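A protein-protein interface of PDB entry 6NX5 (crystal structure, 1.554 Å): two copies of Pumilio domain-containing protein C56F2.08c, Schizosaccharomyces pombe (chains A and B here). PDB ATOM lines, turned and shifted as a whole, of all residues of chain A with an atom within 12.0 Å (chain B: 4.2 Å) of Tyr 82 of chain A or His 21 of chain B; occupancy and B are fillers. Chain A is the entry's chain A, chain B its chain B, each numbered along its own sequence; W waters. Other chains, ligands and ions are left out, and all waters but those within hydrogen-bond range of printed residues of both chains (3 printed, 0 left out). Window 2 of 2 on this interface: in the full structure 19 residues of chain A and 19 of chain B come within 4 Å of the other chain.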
ATOM      1  N   SER A   1      -1.813 -19.188  -0.847  1.00  0.00           N
ATOM      2  CA  SER A   1      -2.097 -19.114  -2.284  1.00  0.00           C
ATOM      3  C   SER A   1      -0.876 -18.583  -3.022  1.00  0.00           C
ATOM      4  O   SER A   1      -0.111 -17.771  -2.486  1.00  0.00           O
ATOM      5  CB  SER A   1      -3.307 -18.235  -2.588  1.00  0.00           C
ATOM      6  OG  SER A   1      -3.114 -16.918  -2.119  1.00  0.00           O
ATOM      7  N   GLY A   2      -0.680 -19.082  -4.237  1.00  0.00           N
ATOM      8  CA  GLY A   2       0.431 -18.627  -5.052  1.00  0.00           C
ATOM      9  C   GLY A   2       1.754 -19.189  -4.568  1.00  0.00           C
ATOM     10  O   GLY A   2       1.830 -20.072  -3.707  1.00  0.00           O
ATOM     11  N   GLY A   3       2.818 -18.657  -5.164  1.00  0.00           N
ATOM     12  CA  GLY A   3       4.166 -19.059  -4.824  1.00  0.00           C
ATOM     13  C   GLY A   3       4.638 -20.250  -5.630  1.00  0.00           C
ATOM     14  O   GLY A   3       3.875 -20.915  -6.340  1.00  0.00           O
ATOM     15  N   LYS A  77       4.743 -25.711 -12.494  1.00  0.00           N
ATOM     16  CA  LYS A  77       4.083 -24.575 -13.093  1.00  0.00           C
ATOM     17  C   LYS A  77       3.367 -23.769 -12.009  1.00  0.00           C
ATOM     18  O   LYS A  77       3.117 -24.280 -10.912  1.00  0.00           O
ATOM     19  CB  LYS A  77       3.074 -25.054 -14.140  1.00  0.00           C
ATOM     20  CG  LYS A  77       3.701 -25.384 -15.496  1.00  0.00           C
ATOM     21  CD  LYS A  77       2.631 -25.840 -16.466  1.00  0.00           C
ATOM     22  CE  LYS A  77       2.271 -27.305 -16.228  1.00  0.00           C
ATOM     23  NZ  LYS A  77       0.954 -27.652 -16.822  1.00  0.00           N
ATOM     24  N   PRO A  78       3.087 -22.494 -12.265  1.00  0.00           N
ATOM     25  CA  PRO A  78       2.268 -21.726 -11.323  1.00  0.00           C
ATOM     26  C   PRO A  78       0.970 -22.453 -11.001  1.00  0.00           C
ATOM     27  O   PRO A  78       0.363 -23.116 -11.848  1.00  0.00           O
ATOM     28  CB  PRO A  78       2.021 -20.403 -12.053  1.00  0.00           C
ATOM     29  CG  PRO A  78       3.135 -20.290 -13.052  1.00  0.00           C
ATOM     30  CD  PRO A  78       3.430 -21.712 -13.467  1.00  0.00           C
ATOM     31  N   SER A  79       0.553 -22.331  -9.755  1.00  0.00           N
ATOM     32  CA  SER A  79      -0.577 -23.086  -9.272  1.00  0.00           C
ATOM     33  C   SER A  79      -1.916 -22.540  -9.774  1.00  0.00           C
ATOM     34  O   SER A  79      -2.049 -21.390 -10.241  1.00  0.00           O
ATOM     35  CB  SER A  79      -0.567 -23.072  -7.753  1.00  0.00           C
ATOM     36  OG  SER A  79      -0.760 -21.741  -7.310  1.00  0.00           O
ATOM     37  N   SER A  80      -2.911 -23.413  -9.712  1.00  0.00           N
ATOM     38  CA  SER A  80      -4.306 -23.013  -9.726  1.00  0.00           C
ATOM     39  C   SER A  80      -4.804 -22.953  -8.292  1.00  0.00           C
ATOM     40  O   SER A  80      -4.492 -23.834  -7.484  1.00  0.00           O
ATOM     41  CB  SER A  80      -5.159 -23.992 -10.529  1.00  0.00           C
ATOM     42  OG  SER A  80      -4.642 -24.156 -11.838  1.00  0.00           O
ATOM     43  N   ASN A  81      -5.571 -21.915  -7.991  1.00  0.00           N
ATOM     44  CA  ASN A  81      -6.114 -21.683  -6.666  1.00  0.00           C
ATOM     45  C   ASN A  81      -7.635 -21.782  -6.729  1.00  0.00           C
ATOM     46  O   ASN A  81      -8.265 -21.322  -7.694  1.00  0.00           O
ATOM     47  CB  ASN A  81      -5.691 -20.313  -6.138  1.00  0.00           C
ATOM     48  CG  ASN A  81      -6.290 -20.009  -4.804  1.00  0.00           C
ATOM     49  OD1 ASN A  81      -7.340 -19.356  -4.713  1.00  0.00           O
ATOM     50  ND2 ASN A  81      -5.643 -20.489  -3.739  1.00  0.00           N
ATOM     51  N   TYR A  82      -8.228 -22.382  -5.696  1.00  0.00           N
ATOM     52  CA  TYR A  82      -9.659 -22.678  -5.647  1.00  0.00           C
ATOM     53  C   TYR A  82     -10.342 -22.050  -4.439  1.00  0.00           C
ATOM     54  O   TYR A  82     -11.423 -22.498  -4.037  1.00  0.00           O
ATOM     55  CB  TYR A  82      -9.868 -24.192  -5.654  1.00  0.00           C
ATOM     56  CG  TYR A  82      -9.202 -24.824  -6.854  1.00  0.00           C
ATOM     57  CD1 TYR A  82      -9.867 -24.905  -8.084  1.00  0.00           C
ATOM     58  CD2 TYR A  82      -7.914 -25.335  -6.769  1.00  0.00           C
ATOM     59  CE1 TYR A  82      -9.254 -25.458  -9.173  1.00  0.00           C
ATOM     60  CE2 TYR A  82      -7.280 -25.881  -7.861  1.00  0.00           C
ATOM     61  CZ  TYR A  82      -7.968 -25.958  -9.065  1.00  0.00           C
ATOM     62  OH  TYR A  82      -7.344 -26.520 -10.149  1.00  0.00           O
ATOM     63  N   GLU A  83      -9.723 -21.043  -3.837  1.00  0.00           N
ATOM     64  CA  GLU A  83     -10.203 -20.484  -2.595  1.00  0.00           C
ATOM     65  C   GLU A  83     -11.093 -19.287  -2.822  1.00  0.00           C
ATOM     66  O   GLU A  83     -11.548 -19.060  -3.934  1.00  0.00           O
ATOM     67  CB  GLU A  83      -9.034 -20.102  -1.703  1.00  0.00           C
ATOM     68  CG  GLU A  83      -8.186 -21.276  -1.298  1.00  0.00           C
ATOM     69  CD  GLU A  83      -7.081 -20.819  -0.392  1.00  0.00           C
ATOM     70  OE1 GLU A  83      -7.204 -21.009   0.841  1.00  0.00           O
ATOM     71  OE2 GLU A  83      -6.113 -20.235  -0.906  1.00  0.00           O
ATOM     72  OXT GLU A  83     -11.372 -18.552  -1.870  1.00  0.00           O
ATOM     73  N   SER B  17      -5.253 -29.892 -14.570  1.00  0.00           N
ATOM     74  CA  SER B  17      -5.516 -29.536 -13.181  1.00  0.00           C
ATOM     75  C   SER B  17      -6.992 -29.698 -12.851  1.00  0.00           C
ATOM     76  O   SER B  17      -7.343 -30.061 -11.721  1.00  0.00           O
ATOM     77  CB  SER B  17      -5.063 -28.109 -12.884  1.00  0.00           C
ATOM     78  OG  SER B  17      -5.760 -27.181 -13.695  1.00  0.00           O
ATOM     79  N   SER B  18      -7.881 -29.457 -13.825  1.00  0.00           N
ATOM     80  CA  SER B  18      -9.301 -29.678 -13.579  1.00  0.00           C
ATOM     81  C   SER B  18      -9.584 -31.137 -13.238  1.00  0.00           C
ATOM     82  O   SER B  18     -10.376 -31.427 -12.339  1.00  0.00           O
ATOM     83  CB  SER B  18     -10.117 -29.247 -14.797  1.00  0.00           C
ATOM     84  OG  SER B  18     -11.447 -29.723 -14.700  1.00  0.00           O
ATOM     85  N   ALA B  19      -8.929 -32.072 -13.935  1.00  0.00           N
ATOM     86  CA  ALA B  19      -9.129 -33.489 -13.633  1.00  0.00           C
ATOM     87  C   ALA B  19      -8.615 -33.853 -12.244  1.00  0.00           C
ATOM     88  O   ALA B  19      -9.248 -34.639 -11.535  1.00  0.00           O
ATOM     89  CB  ALA B  19      -8.452 -34.360 -14.695  1.00  0.00           C
ATOM     90  N   ILE B  20      -7.469 -33.295 -11.845  1.00  0.00           N
ATOM     91  CA  ILE B  20      -6.957 -33.530 -10.494  1.00  0.00           C
ATOM     92  C   ILE B  20      -7.904 -32.936  -9.459  1.00  0.00           C
ATOM     93  O   ILE B  20      -8.186 -33.559  -8.418  1.00  0.00           O
ATOM     94  CB  ILE B  20      -5.535 -32.948 -10.373  1.00  0.00           C
ATOM     95  CG1 ILE B  20      -4.587 -33.647 -11.361  1.00  0.00           C
ATOM     96  CG2 ILE B  20      -5.036 -32.999  -8.920  1.00  0.00           C
ATOM     97  CD1 ILE B  20      -4.427 -35.111 -11.084  1.00  0.00           C
ATOM     98  N   HIS B  21      -8.374 -31.706  -9.693  1.00  0.00           N
ATOM     99  CA  HIS B  21      -9.294 -31.084  -8.748  1.00  0.00           C
ATOM    100  C   HIS B  21     -10.546 -31.939  -8.556  1.00  0.00           C
ATOM    101  O   HIS B  21     -10.995 -32.148  -7.428  1.00  0.00           O
ATOM    102  CB  HIS B  21      -9.688 -29.681  -9.210  1.00  0.00           C
ATOM    103  CG  HIS B  21     -10.543 -28.966  -8.210  1.00  0.00           C
ATOM    104  ND1 HIS B  21     -11.922 -29.048  -8.206  1.00  0.00           N
ATOM    105  CD2 HIS B  21     -10.208 -28.202  -7.144  1.00  0.00           C
ATOM    106  CE1 HIS B  21     -12.398 -28.344  -7.194  1.00  0.00           C
ATOM    107  NE2 HIS B  21     -11.379 -27.817  -6.536  1.00  0.00           N
ATOM    108  N   ALA B  22     -11.128 -32.432  -9.650  1.00  0.00           N
ATOM    109  CA  ALA B  22     -12.323 -33.275  -9.550  1.00  0.00           C
ATOM    110  C   ALA B  22     -12.043 -34.555  -8.766  1.00  0.00           C
ATOM    111  O   ALA B  22     -12.861 -34.984  -7.938  1.00  0.00           O
ATOM    112  CB  ALA B  22     -12.834 -33.609 -10.955  1.00  0.00           C
ATOM    113  N   LEU B  23     -10.891 -35.176  -9.011  1.00  0.00           N
ATOM    114  CA  LEU B  23     -10.579 -36.424  -8.342  1.00  0.00           C
ATOM    115  C   LEU B  23     -10.408 -36.200  -6.849  1.00  0.00           C
ATOM    116  O   LEU B  23     -11.011 -36.906  -6.026  1.00  0.00           O
ATOM    117  CB  LEU B  23      -9.318 -37.029  -8.949  1.00  0.00           C
ATOM    118  CG  LEU B  23      -8.844 -38.349  -8.367  1.00  0.00           C
ATOM    119  CD1 LEU B  23      -9.810 -39.452  -8.744  1.00  0.00           C
ATOM    120  CD2 LEU B  23      -7.456 -38.638  -8.897  1.00  0.00           C
ATOM    121  N   PHE B  24      -9.622 -35.192  -6.484  1.00  0.00           N
ATOM    122  CA  PHE B  24      -9.266 -35.022  -5.087  1.00  0.00           C
ATOM    123  C   PHE B  24     -10.328 -34.274  -4.295  1.00  0.00           C
ATOM    124  O   PHE B  24     -10.336 -34.368  -3.057  1.00  0.00           O
ATOM    125  CB  PHE B  24      -7.881 -34.353  -5.007  1.00  0.00           C
ATOM    126  CG  PHE B  24      -6.765 -35.313  -5.298  1.00  0.00           C
ATOM    127  CD1 PHE B  24      -6.224 -36.079  -4.280  1.00  0.00           C
ATOM    128  CD2 PHE B  24      -6.330 -35.523  -6.602  1.00  0.00           C
ATOM    129  CE1 PHE B  24      -5.246 -37.030  -4.554  1.00  0.00           C
ATOM    130  CE2 PHE B  24      -5.340 -36.455  -6.871  1.00  0.00           C
ATOM    131  CZ  PHE B  24      -4.799 -37.204  -5.853  1.00  0.00           C
ATOM    132  N   SER B  25     -11.237 -33.568  -4.961  1.00  0.00           N
ATOM    133  CA  SER B  25     -12.276 -32.847  -4.232  1.00  0.00           C
ATOM    134  C   SER B  25     -13.267 -33.774  -3.545  1.00  0.00           C
ATOM    135  O   SER B  25     -14.007 -33.322  -2.667  1.00  0.00           O
ATOM    136  CB  SER B  25     -13.017 -31.899  -5.174  1.00  0.00           C
ATOM    137  OG  SER B  25     -12.203 -30.765  -5.407  1.00  0.00           O
ATOM    138  N   VAL B  30      -9.926 -28.766  -1.704  1.00  0.00           N
ATOM    139  CA  VAL B  30      -8.664 -28.514  -2.402  1.00  0.00           C
ATOM    140  C   VAL B  30      -8.426 -27.014  -2.502  1.00  0.00           C
ATOM    141  O   VAL B  30      -9.219 -26.290  -3.118  1.00  0.00           O
ATOM    142  CB  VAL B  30      -8.677 -29.142  -3.799  1.00  0.00           C
ATOM    143  CG1 VAL B  30      -7.413 -28.718  -4.562  1.00  0.00           C
ATOM    144  CG2 VAL B  30      -8.786 -30.661  -3.670  1.00  0.00           C
ATOM    145  N   LYS B  31      -7.317 -26.547  -1.925  1.00  0.00           N
ATOM    146  CA  LYS B  31      -7.023 -25.117  -1.964  1.00  0.00           C
ATOM    147  C   LYS B  31      -6.199 -24.740  -3.186  1.00  0.00           C
ATOM    148  O   LYS B  31      -6.447 -23.706  -3.804  1.00  0.00           O
ATOM    149  CB  LYS B  31      -6.264 -24.693  -0.709  1.00  0.00           C
ATOM    150  CG  LYS B  31      -7.080 -24.767   0.595  1.00  0.00           C
ATOM    151  CD  LYS B  31      -6.295 -24.248   1.819  1.00  0.00           C
ATOM    152  CE  LYS B  31      -4.979 -24.985   2.040  1.00  0.00           C
ATOM    153  NZ  LYS B  31      -4.267 -24.442   3.275  1.00  0.00           N
ATOM    154  N   ILE B  33      -3.445 -26.398  -6.528  1.00  0.00           N
ATOM    155  CA  ILE B  33      -2.818 -27.500  -7.256  1.00  0.00           C
ATOM    156  C   ILE B  33      -1.655 -26.931  -8.052  1.00  0.00           C
ATOM    157  O   ILE B  33      -1.826 -25.944  -8.781  1.00  0.00           O
ATOM    158  CB  ILE B  33      -3.815 -28.211  -8.199  1.00  0.00           C
ATOM    159  CG1 ILE B  33      -4.910 -28.898  -7.385  1.00  0.00           C
ATOM    160  CG2 ILE B  33      -3.091 -29.230  -9.106  1.00  0.00           C
ATOM    161  CD1 ILE B  33      -6.080 -29.424  -8.235  1.00  0.00           C
HETATM  162  O   HOH W   1      -2.688 -26.270 -11.716  1.00  0.00           O
HETATM  163  O   HOH W   2      -8.340 -26.299 -12.523  1.00  0.00           O
HETATM  164  O   HOH W   3     -10.977 -23.797  -1.429  1.00  0.00           O
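O of Lys 31 of chain B sits at hydrogen-bond distance from N of Tyr 82 of chain A, at 2.9 Å. The backbone NH (N) of Ser 80 of chain A sits at hydrogen-bond distance from the backbone carbonyl oxygen (O) of Ile 33 of chain B (2.9 Å). The backbone carbonyl oxygen of Lys 31 of chain B lies within hydrogen-bond range of the side-chain amide nitrogen of Asn 81 of chain A (3.3 Å).
The side-chain amide nitrogen of Asn 81 of chain A lies within hydrogen-bond range of the side-chain carboxylate of Glu 83 of chain A (2.9 Å). The backbone carbonyl oxygen of His 21 of chain B sits at hydrogen-bond distance from the side-chain hydroxyl of Ser 25 of chain B, 2.7 Å away.
Among the printed residues, merely in contact across the chains: Ser 79 of chain A with Ile 33 of chain B, Tyr 82 of chain A with Val 30 of chain B, Tyr 82 of chain A with His 21 of chain B, Glu 83 of chain A with Lys 31 of chain B, Tyr 82 of chain A with Ile 33 of chain B, Ser 80 of chain A with Ser 17 of chain B and Tyr 82 of chain A with Ser 17 of chain B.
Of the printed residues of chain B, Tyr 82 of chain A touches Ser 17, His 21, Val 30, Lys 31 and Ile 33. His 21 of chain B touches just one residue of chain A: Tyr 82 (3.4 Å). Val 30 of chain B touches just one residue of chain A: Tyr 82 (3.4 Å). Of the printed residues of chain A, Lys 31 of chain B touches Asn 81 (3.3 Å), Tyr 82 (2.9 Å) and Glu 83 (3.5 Å). Of the printed residues of chain B, Glu 83 of chain A touches Lys 31 (3.5 Å). Of the printed residues of chain A, Ile 33 of chain B touches Ser 79 (3.2 Å), Ser 80 (2.9 Å) and Tyr 82 (3.7 Å). Of the printed residues of chain B, Ser 79 of chain A touches Ile 33 (3.2 Å). The nearest printed residue of chain B that does not touch Tyr 82 of chain A is Ser 18 of chain B (4.7 Å).
Of the 12 printed residues of chain B, 5 touch a printed residue of chain A. Printed residues of chain B that touch a printed residue of chain A: Ser 17, His 21, Val 30, Lys 31 and Ile 33. Along chain B the printed residues that touch a printed residue of chain A span positions 17 to 33. Of the 10 printed residues of chain A, 5 touch a printed residue of chain B. Along chain A the printed residues that touch a printed residue of chain B span positions 79 to 83. Among the printed residues, 10 pairs touch across the chains. Among the printed residues, no Asp or Glu carboxylate lies within 4 Å of a Lys or Arg side-chain nitrogen of the other chain.
No position is printed for both chains.
Water W2 lies within hydrogen-bond range of the side-chain hydroxyl of Tyr 82 of chain A (2.6 Å), the side-chain hydroxyl of Ser 17 of chain B (3.0 Å) and the backbone NH of Ser 18 of chain B (3.4 Å). Water W1 bridges OG of Ser 80 of chain A (2.9 Å) and O of Ile 33 of chain B (3.1 Å). Water W3 bridges O of Tyr 82 of chain A and O of Val 30 of chain B.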
